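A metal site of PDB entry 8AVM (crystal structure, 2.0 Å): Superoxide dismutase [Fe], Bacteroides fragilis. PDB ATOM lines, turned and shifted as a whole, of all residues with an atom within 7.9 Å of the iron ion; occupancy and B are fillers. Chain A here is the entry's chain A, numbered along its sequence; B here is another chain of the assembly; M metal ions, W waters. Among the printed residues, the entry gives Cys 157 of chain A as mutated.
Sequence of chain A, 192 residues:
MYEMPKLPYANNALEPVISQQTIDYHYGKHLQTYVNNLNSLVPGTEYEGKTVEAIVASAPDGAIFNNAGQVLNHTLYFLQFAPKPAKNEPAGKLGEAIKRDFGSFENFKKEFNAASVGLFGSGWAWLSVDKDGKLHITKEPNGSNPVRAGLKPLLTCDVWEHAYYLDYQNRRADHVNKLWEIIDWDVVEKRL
OD1 of Asp 158 lies within hydrogen-bond range of N of Trp 160. OE2 of Glu 161 of chain B sits at hydrogen-bond distance from ND1 of His 162, at 2.9 Å. The indole nitrogen (NE1) of Trp 124 sits at hydrogen-bond distance from the side-chain amide oxygen (OE1) of Gln 70 (2.8 Å). NE1 of Trp 124 sits close to O of Asn 142 (3.1 Å). The indole nitrogen (NE1) of Trp 124 sits close to the side-chain amide nitrogen (ND2) of Asn 73 (3.2 Å). The backbone NH (N) of Leu 31 sits at hydrogen-bond distance from the backbone carbonyl oxygen (O) of His 26 (3.1 Å). ND1 of His 74 sits at hydrogen-bond distance from O of Gln 70, at 2.7 Å.
Trp 124 touches the iron ion (CZ2 to FE, 3.98 Å). Five residues have an atom within 4 Å of the iron ion: His 26, His 74, Trp 124, Asp 158 and His 162.
The iron ion is bound by OD2 of Asp 158 (1.9 Å), water W1 (2.0 Å), NE2 of His 162 (2.1 Å), NE2 of His 74 (2.1 Å) and NE2 of His 26 (2.2 Å).
Water W1 lies within hydrogen-bond range of the side-chain carboxylate of Asp 158 (3.0 Å) and the side-chain amide nitrogen of Gln 70 (3.0 Å).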
ATOM      1  N   HIS A  26       1.333  30.939   5.907  1.00  0.00           N
ATOM      2  CA  HIS A  26       0.627  30.257   4.818  1.00  0.00           C
ATOM      3  C   HIS A  26       1.436  29.016   4.396  1.00  0.00           C
ATOM      4  O   HIS A  26       0.907  27.916   4.317  1.00  0.00           O
ATOM      5  CB  HIS A  26       0.301  31.242   3.686  1.00  0.00           C
ATOM      6  CG  HIS A  26      -0.756  30.747   2.777  1.00  0.00           C
ATOM      7  ND1 HIS A  26      -1.174  31.495   1.687  1.00  0.00           N
ATOM      8  CD2 HIS A  26      -1.483  29.588   2.759  1.00  0.00           C
ATOM      9  CE1 HIS A  26      -2.147  30.808   1.051  1.00  0.00           C
ATOM     10  NE2 HIS A  26      -2.346  29.659   1.685  1.00  0.00           N
ATOM     11  N   TYR A  27       2.721  29.227   4.115  1.00  0.00           N
ATOM     12  CA  TYR A  27       3.601  28.155   3.715  1.00  0.00           C
ATOM     13  C   TYR A  27       4.121  27.413   4.947  1.00  0.00           C
ATOM     14  O   TYR A  27       4.002  26.187   5.049  1.00  0.00           O
ATOM     15  CB  TYR A  27       4.747  28.741   2.879  1.00  0.00           C
ATOM     16  CG  TYR A  27       5.858  27.777   2.568  1.00  0.00           C
ATOM     17  CD1 TYR A  27       5.749  26.918   1.481  1.00  0.00           C
ATOM     18  CD2 TYR A  27       6.988  27.691   3.371  1.00  0.00           C
ATOM     19  CE1 TYR A  27       6.773  26.043   1.162  1.00  0.00           C
ATOM     20  CE2 TYR A  27       8.026  26.828   3.059  1.00  0.00           C
ATOM     21  CZ  TYR A  27       7.905  25.987   1.967  1.00  0.00           C
ATOM     22  OH  TYR A  27       8.906  25.102   1.651  1.00  0.00           O
ATOM     23  N   HIS A  30       0.379  26.436   7.511  1.00  0.00           N
ATOM     24  CA  HIS A  30      -0.769  25.792   6.864  1.00  0.00           C
ATOM     25  C   HIS A  30      -0.294  24.669   5.937  1.00  0.00           C
ATOM     26  O   HIS A  30      -0.804  23.544   6.016  1.00  0.00           O
ATOM     27  CB  HIS A  30      -1.650  26.803   6.113  1.00  0.00           C
ATOM     28  CG  HIS A  30      -2.451  27.735   6.942  1.00  0.00           C
ATOM     29  ND1 HIS A  30      -3.728  27.511   7.407  1.00  0.00           N
ATOM     30  CD2 HIS A  30      -2.111  29.002   7.353  1.00  0.00           C
ATOM     31  CE1 HIS A  30      -4.130  28.556   8.145  1.00  0.00           C
ATOM     32  NE2 HIS A  30      -3.147  29.479   8.123  1.00  0.00           N
ATOM     33  N   LEU A  31       0.663  24.961   5.046  1.00  0.00           N
ATOM     34  CA  LEU A  31       1.056  23.939   4.084  1.00  0.00           C
ATOM     35  C   LEU A  31       1.760  22.811   4.817  1.00  0.00           C
ATOM     36  O   LEU A  31       1.490  21.631   4.557  1.00  0.00           O
ATOM     37  CB  LEU A  31       1.901  24.519   2.949  1.00  0.00           C
ATOM     38  CG  LEU A  31       2.446  23.482   1.972  1.00  0.00           C
ATOM     39  CD1 LEU A  31       1.299  22.595   1.415  1.00  0.00           C
ATOM     40  CD2 LEU A  31       3.189  24.147   0.836  1.00  0.00           C
ATOM     41  N   TYR A  34      -0.711  20.487   6.202  1.00  0.00           N
ATOM     42  CA  TYR A  34      -1.340  19.626   5.201  1.00  0.00           C
ATOM     43  C   TYR A  34      -0.398  18.477   4.833  1.00  0.00           C
ATOM     44  O   TYR A  34      -0.811  17.325   4.683  1.00  0.00           O
ATOM     45  CB  TYR A  34      -1.763  20.436   3.972  1.00  0.00           C
ATOM     46  CG  TYR A  34      -2.855  21.447   4.230  1.00  0.00           C
ATOM     47  CD1 TYR A  34      -4.040  21.088   4.840  1.00  0.00           C
ATOM     48  CD2 TYR A  34      -2.722  22.759   3.770  1.00  0.00           C
ATOM     49  CE1 TYR A  34      -5.058  22.017   5.040  1.00  0.00           C
ATOM     50  CE2 TYR A  34      -3.736  23.683   3.946  1.00  0.00           C
ATOM     51  CZ  TYR A  34      -4.891  23.316   4.591  1.00  0.00           C
ATOM     52  OH  TYR A  34      -5.919  24.189   4.741  1.00  0.00           O
ATOM     53  N   GLN A  70      -5.165  20.168  -0.787  1.00  0.00           N
ATOM     54  CA  GLN A  70      -4.569  21.382  -0.289  1.00  0.00           C
ATOM     55  C   GLN A  70      -3.058  21.365  -0.545  1.00  0.00           C
ATOM     56  O   GLN A  70      -2.459  22.417  -0.820  1.00  0.00           O
ATOM     57  CB  GLN A  70      -4.916  21.581   1.187  1.00  0.00           C
ATOM     58  CG  GLN A  70      -6.341  22.077   1.397  1.00  0.00           C
ATOM     59  CD  GLN A  70      -6.581  23.459   0.827  1.00  0.00           C
ATOM     60  OE1 GLN A  70      -6.811  23.615  -0.377  1.00  0.00           O
ATOM     61  NE2 GLN A  70      -6.581  24.470   1.697  1.00  0.00           N
ATOM     62  N   ASN A  73      -2.850  22.170  -4.324  1.00  0.00           N
ATOM     63  CA  ASN A  73      -3.237  23.563  -4.526  1.00  0.00           C
ATOM     64  C   ASN A  73      -2.083  24.491  -4.094  1.00  0.00           C
ATOM     65  O   ASN A  73      -1.713  25.394  -4.832  1.00  0.00           O
ATOM     66  CB  ASN A  73      -4.536  23.907  -3.774  1.00  0.00           C
ATOM     67  CG  ASN A  73      -5.785  23.437  -4.482  1.00  0.00           C
ATOM     68  OD1 ASN A  73      -5.836  23.406  -5.716  1.00  0.00           O
ATOM     69  ND2 ASN A  73      -6.833  23.157  -3.702  1.00  0.00           N
ATOM     70  N   HIS A  74      -1.555  24.304  -2.886  1.00  0.00           N
ATOM     71  CA  HIS A  74      -0.585  25.252  -2.365  1.00  0.00           C
ATOM     72  C   HIS A  74       0.748  25.108  -3.077  1.00  0.00           C
ATOM     73  O   HIS A  74       1.496  26.087  -3.226  1.00  0.00           O
ATOM     74  CB  HIS A  74      -0.405  25.109  -0.865  1.00  0.00           C
ATOM     75  CG  HIS A  74      -1.527  25.624  -0.026  1.00  0.00           C
ATOM     76  ND1 HIS A  74      -2.606  24.822   0.312  1.00  0.00           N
ATOM     77  CD2 HIS A  74      -1.794  26.851   0.451  1.00  0.00           C
ATOM     78  CE1 HIS A  74      -3.468  25.537   1.021  1.00  0.00           C
ATOM     79  NE2 HIS A  74      -3.005  26.782   1.121  1.00  0.00           N
ATOM     80  N   TYR A  77       0.294  26.972  -6.291  1.00  0.00           N
ATOM     81  CA  TYR A  77       0.141  28.351  -5.892  1.00  0.00           C
ATOM     82  C   TYR A  77       1.488  29.000  -5.630  1.00  0.00           C
ATOM     83  O   TYR A  77       1.835  30.008  -6.258  1.00  0.00           O
ATOM     84  CB  TYR A  77      -0.731  28.425  -4.642  1.00  0.00           C
ATOM     85  CG  TYR A  77      -1.007  29.786  -4.051  1.00  0.00           C
ATOM     86  CD1 TYR A  77      -1.848  30.713  -4.666  1.00  0.00           C
ATOM     87  CD2 TYR A  77      -0.503  30.116  -2.802  1.00  0.00           C
ATOM     88  CE1 TYR A  77      -2.147  31.930  -4.066  1.00  0.00           C
ATOM     89  CE2 TYR A  77      -0.820  31.325  -2.186  1.00  0.00           C
ATOM     90  CZ  TYR A  77      -1.640  32.231  -2.807  1.00  0.00           C
ATOM     91  OH  TYR A  77      -1.939  33.372  -2.141  1.00  0.00           O
ATOM     92  N   PHE A  78       2.234  28.493  -4.674  1.00  0.00           N
ATOM     93  CA  PHE A  78       3.430  29.198  -4.280  1.00  0.00           C
ATOM     94  C   PHE A  78       4.447  29.210  -5.410  1.00  0.00           C
ATOM     95  O   PHE A  78       5.202  30.182  -5.560  1.00  0.00           O
ATOM     96  CB  PHE A  78       4.017  28.591  -3.019  1.00  0.00           C
ATOM     97  CG  PHE A  78       3.221  28.846  -1.774  1.00  0.00           C
ATOM     98  CD1 PHE A  78       3.016  30.147  -1.342  1.00  0.00           C
ATOM     99  CD2 PHE A  78       2.697  27.812  -1.023  1.00  0.00           C
ATOM    100  CE1 PHE A  78       2.297  30.390  -0.189  1.00  0.00           C
ATOM    101  CE2 PHE A  78       2.005  28.049   0.143  1.00  0.00           C
ATOM    102  CZ  PHE A  78       1.802  29.346   0.552  1.00  0.00           C
ATOM    103  N   GLY A 123     -11.922  28.455  -0.748  1.00  0.00           N
ATOM    104  CA  GLY A 123     -11.720  27.752  -1.988  1.00  0.00           C
ATOM    105  C   GLY A 123     -10.606  28.367  -2.838  1.00  0.00           C
ATOM    106  O   GLY A 123      -9.798  29.146  -2.356  1.00  0.00           O
ATOM    107  N   TRP A 124     -10.589  27.964  -4.108  1.00  0.00           N
ATOM    108  CA  TRP A 124      -9.592  28.310  -5.101  1.00  0.00           C
ATOM    109  C   TRP A 124     -10.272  28.666  -6.425  1.00  0.00           C
ATOM    110  O   TRP A 124     -11.104  27.909  -6.924  1.00  0.00           O
ATOM    111  CB  TRP A 124      -8.666  27.119  -5.324  1.00  0.00           C
ATOM    112  CG  TRP A 124      -8.019  26.635  -4.075  1.00  0.00           C
ATOM    113  CD1 TRP A 124      -8.570  25.932  -3.045  1.00  0.00           C
ATOM    114  CD2 TRP A 124      -6.676  26.937  -3.683  1.00  0.00           C
ATOM    115  NE1 TRP A 124      -7.667  25.762  -2.042  1.00  0.00           N
ATOM    116  CE2 TRP A 124      -6.496  26.375  -2.405  1.00  0.00           C
ATOM    117  CE3 TRP A 124      -5.633  27.636  -4.307  1.00  0.00           C
ATOM    118  CZ2 TRP A 124      -5.284  26.468  -1.741  1.00  0.00           C
ATOM    119  CZ3 TRP A 124      -4.436  27.713  -3.641  1.00  0.00           C
ATOM    120  CH2 TRP A 124      -4.269  27.143  -2.381  1.00  0.00           C
ATOM    121  N   ASN A 142     -13.151  24.778  -0.940  1.00  0.00           N
ATOM    122  CA  ASN A 142     -12.355  24.176   0.126  1.00  0.00           C
ATOM    123  C   ASN A 142     -11.036  23.670  -0.441  1.00  0.00           C
ATOM    124  O   ASN A 142     -10.204  24.459  -0.906  1.00  0.00           O
ATOM    125  CB  ASN A 142     -13.217  23.157   0.892  1.00  0.00           C
ATOM    126  CG  ASN A 142     -14.365  23.832   1.633  1.00  0.00           C
ATOM    127  OD1 ASN A 142     -14.299  25.026   1.930  1.00  0.00           O
ATOM    128  ND2 ASN A 142     -15.432  23.111   1.876  1.00  0.00           N
ATOM    129  N   CYS A 157      -5.849  31.336  -7.647  1.00  0.00           N
ATOM    130  CA  CYS A 157      -5.899  32.244  -6.532  1.00  0.00           C
ATOM    131  C   CYS A 157      -6.553  31.552  -5.336  1.00  0.00           C
ATOM    132  O   CYS A 157      -7.659  31.057  -5.420  1.00  0.00           O
ATOM    133  CB  CYS A 157      -6.658  33.516  -6.932  1.00  0.00           C
ATOM    134  SG  CYS A 157      -7.060  34.573  -5.499  1.00  0.00           S
ATOM    135  N   ASP A 158      -5.824  31.507  -4.218  1.00  0.00           N
ATOM    136  CA  ASP A 158      -6.290  30.936  -2.980  1.00  0.00           C
ATOM    137  C   ASP A 158      -7.135  31.994  -2.291  1.00  0.00           C
ATOM    138  O   ASP A 158      -6.582  33.036  -1.911  1.00  0.00           O
ATOM    139  CB  ASP A 158      -5.123  30.576  -2.051  1.00  0.00           C
ATOM    140  CG  ASP A 158      -5.478  29.909  -0.736  1.00  0.00           C
ATOM    141  OD1 ASP A 158      -6.680  29.664  -0.500  1.00  0.00           O
ATOM    142  OD2 ASP A 158      -4.546  29.593   0.005  1.00  0.00           O
ATOM    143  N   VAL A 159      -8.437  31.723  -2.117  1.00  0.00           N
ATOM    144  CA  VAL A 159      -9.292  32.713  -1.484  1.00  0.00           C
ATOM    145  C   VAL A 159      -9.745  32.271  -0.084  1.00  0.00           C
ATOM    146  O   VAL A 159     -10.606  32.933   0.500  1.00  0.00           O
ATOM    147  CB  VAL A 159     -10.492  33.140  -2.354  1.00  0.00           C
ATOM    148  CG1 VAL A 159     -10.036  33.799  -3.633  1.00  0.00           C
ATOM    149  CG2 VAL A 159     -11.444  31.998  -2.638  1.00  0.00           C
ATOM    150  N   TRP A 160      -9.132  31.217   0.467  1.00  0.00           N
ATOM    151  CA  TRP A 160      -9.152  31.019   1.897  1.00  0.00           C
ATOM    152  C   TRP A 160      -8.670  32.327   2.530  1.00  0.00           C
ATOM    153  O   TRP A 160      -7.697  32.932   2.095  1.00  0.00           O
ATOM    154  CB  TRP A 160      -8.234  29.870   2.336  1.00  0.00           C
ATOM    155  CG  TRP A 160      -8.714  28.496   2.007  1.00  0.00           C
ATOM    156  CD1 TRP A 160      -8.944  27.978   0.765  1.00  0.00           C
ATOM    157  CD2 TRP A 160      -8.986  27.450   2.942  1.00  0.00           C
ATOM    158  NE1 TRP A 160      -9.333  26.677   0.874  1.00  0.00           N
ATOM    159  CE2 TRP A 160      -9.367  26.323   2.186  1.00  0.00           C
ATOM    160  CE3 TRP A 160      -8.925  27.345   4.339  1.00  0.00           C
ATOM    161  CZ2 TRP A 160      -9.738  25.120   2.799  1.00  0.00           C
ATOM    162  CZ3 TRP A 160      -9.222  26.133   4.938  1.00  0.00           C
ATOM    163  CH2 TRP A 160      -9.644  25.039   4.179  1.00  0.00           C
ATOM    164  N   GLU A 161      -9.326  32.714   3.603  1.00  0.00           N
ATOM    165  CA  GLU A 161      -8.982  34.021   4.200  1.00  0.00           C
ATOM    166  C   GLU A 161      -7.524  34.095   4.687  1.00  0.00           C
ATOM    167  O   GLU A 161      -6.903  35.148   4.650  1.00  0.00           O
ATOM    168  CB  GLU A 161      -9.978  34.341   5.317  1.00  0.00           C
ATOM    169  CG  GLU A 161     -11.349  34.748   4.730  1.00  0.00           C
ATOM    170  CD  GLU A 161     -12.457  34.982   5.744  1.00  0.00           C
ATOM    171  OE1 GLU A 161     -12.562  34.195   6.726  1.00  0.00           O
ATOM    172  OE2 GLU A 161     -13.135  35.997   5.620  1.00  0.00           O
ATOM    173  N   HIS A 162      -6.977  32.964   5.170  1.00  0.00           N
ATOM    174  CA  HIS A 162      -5.599  32.933   5.629  1.00  0.00           C
ATOM    175  C   HIS A 162      -4.632  33.432   4.556  1.00  0.00           C
ATOM    176  O   HIS A 162      -3.514  33.858   4.877  1.00  0.00           O
ATOM    177  CB  HIS A 162      -5.177  31.538   6.125  1.00  0.00           C
ATOM    178  CG  HIS A 162      -5.112  30.466   5.083  1.00  0.00           C
ATOM    179  ND1 HIS A 162      -5.855  29.320   5.224  1.00  0.00           N
ATOM    180  CD2 HIS A 162      -4.412  30.303   3.942  1.00  0.00           C
ATOM    181  CE1 HIS A 162      -5.603  28.522   4.194  1.00  0.00           C
ATOM    182  NE2 HIS A 162      -4.743  29.081   3.396  1.00  0.00           N
ATOM    183  N   ALA A 163      -5.063  33.403   3.278  1.00  0.00           N
ATOM    184  CA  ALA A 163      -4.140  33.727   2.195  1.00  0.00           C
ATOM    185  C   ALA A 163      -3.885  35.248   2.163  1.00  0.00           C
ATOM    186  O   ALA A 163      -2.874  35.705   1.612  1.00  0.00           O
ATOM    187  CB  ALA A 163      -4.678  33.225   0.863  1.00  0.00           C
ATOM    188  N   TYR A 164      -4.847  36.011   2.698  1.00  0.00           N
ATOM    189  CA  TYR A 164      -4.817  37.462   2.561  1.00  0.00           C
ATOM    190  C   TYR A 164      -5.143  38.231   3.842  1.00  0.00           C
ATOM    191  O   TYR A 164      -4.949  39.446   3.905  1.00  0.00           O
ATOM    192  CB  TYR A 164      -5.749  37.913   1.436  1.00  0.00           C
ATOM    193  CG  TYR A 164      -7.213  37.564   1.557  1.00  0.00           C
ATOM    194  CD1 TYR A 164      -8.093  38.319   2.313  1.00  0.00           C
ATOM    195  CD2 TYR A 164      -7.720  36.458   0.889  1.00  0.00           C
ATOM    196  CE1 TYR A 164      -9.453  38.003   2.378  1.00  0.00           C
ATOM    197  CE2 TYR A 164      -9.072  36.113   0.987  1.00  0.00           C
ATOM    198  CZ  TYR A 164      -9.941  36.873   1.714  1.00  0.00           C
ATOM    199  OH  TYR A 164     -11.318  36.539   1.735  1.00  0.00           O
ATOM    200  N   GLU B 161     -12.047  31.819   9.117  1.00  0.00           N
ATOM    201  CA  GLU B 161     -10.761  32.318   9.589  1.00  0.00           C
ATOM    202  C   GLU B 161     -10.797  33.769  10.052  1.00  0.00           C
ATOM    203  O   GLU B 161     -10.084  34.106  10.996  1.00  0.00           O
ATOM    204  CB  GLU B 161      -9.691  32.073   8.530  1.00  0.00           C
ATOM    205  CG  GLU B 161      -9.280  30.624   8.444  1.00  0.00           C
ATOM    206  CD  GLU B 161      -8.313  30.227   7.342  1.00  0.00           C
ATOM    207  OE1 GLU B 161      -8.490  30.686   6.241  1.00  0.00           O
ATOM    208  OE2 GLU B 161      -7.457  29.349   7.627  1.00  0.00           O
HETATM  209 FE    FE M   1      -4.189  28.480   1.508  1.00  0.00          FE
HETATM  210  O   HOH W   1      -5.832  27.393   1.318  1.00  0.00           O
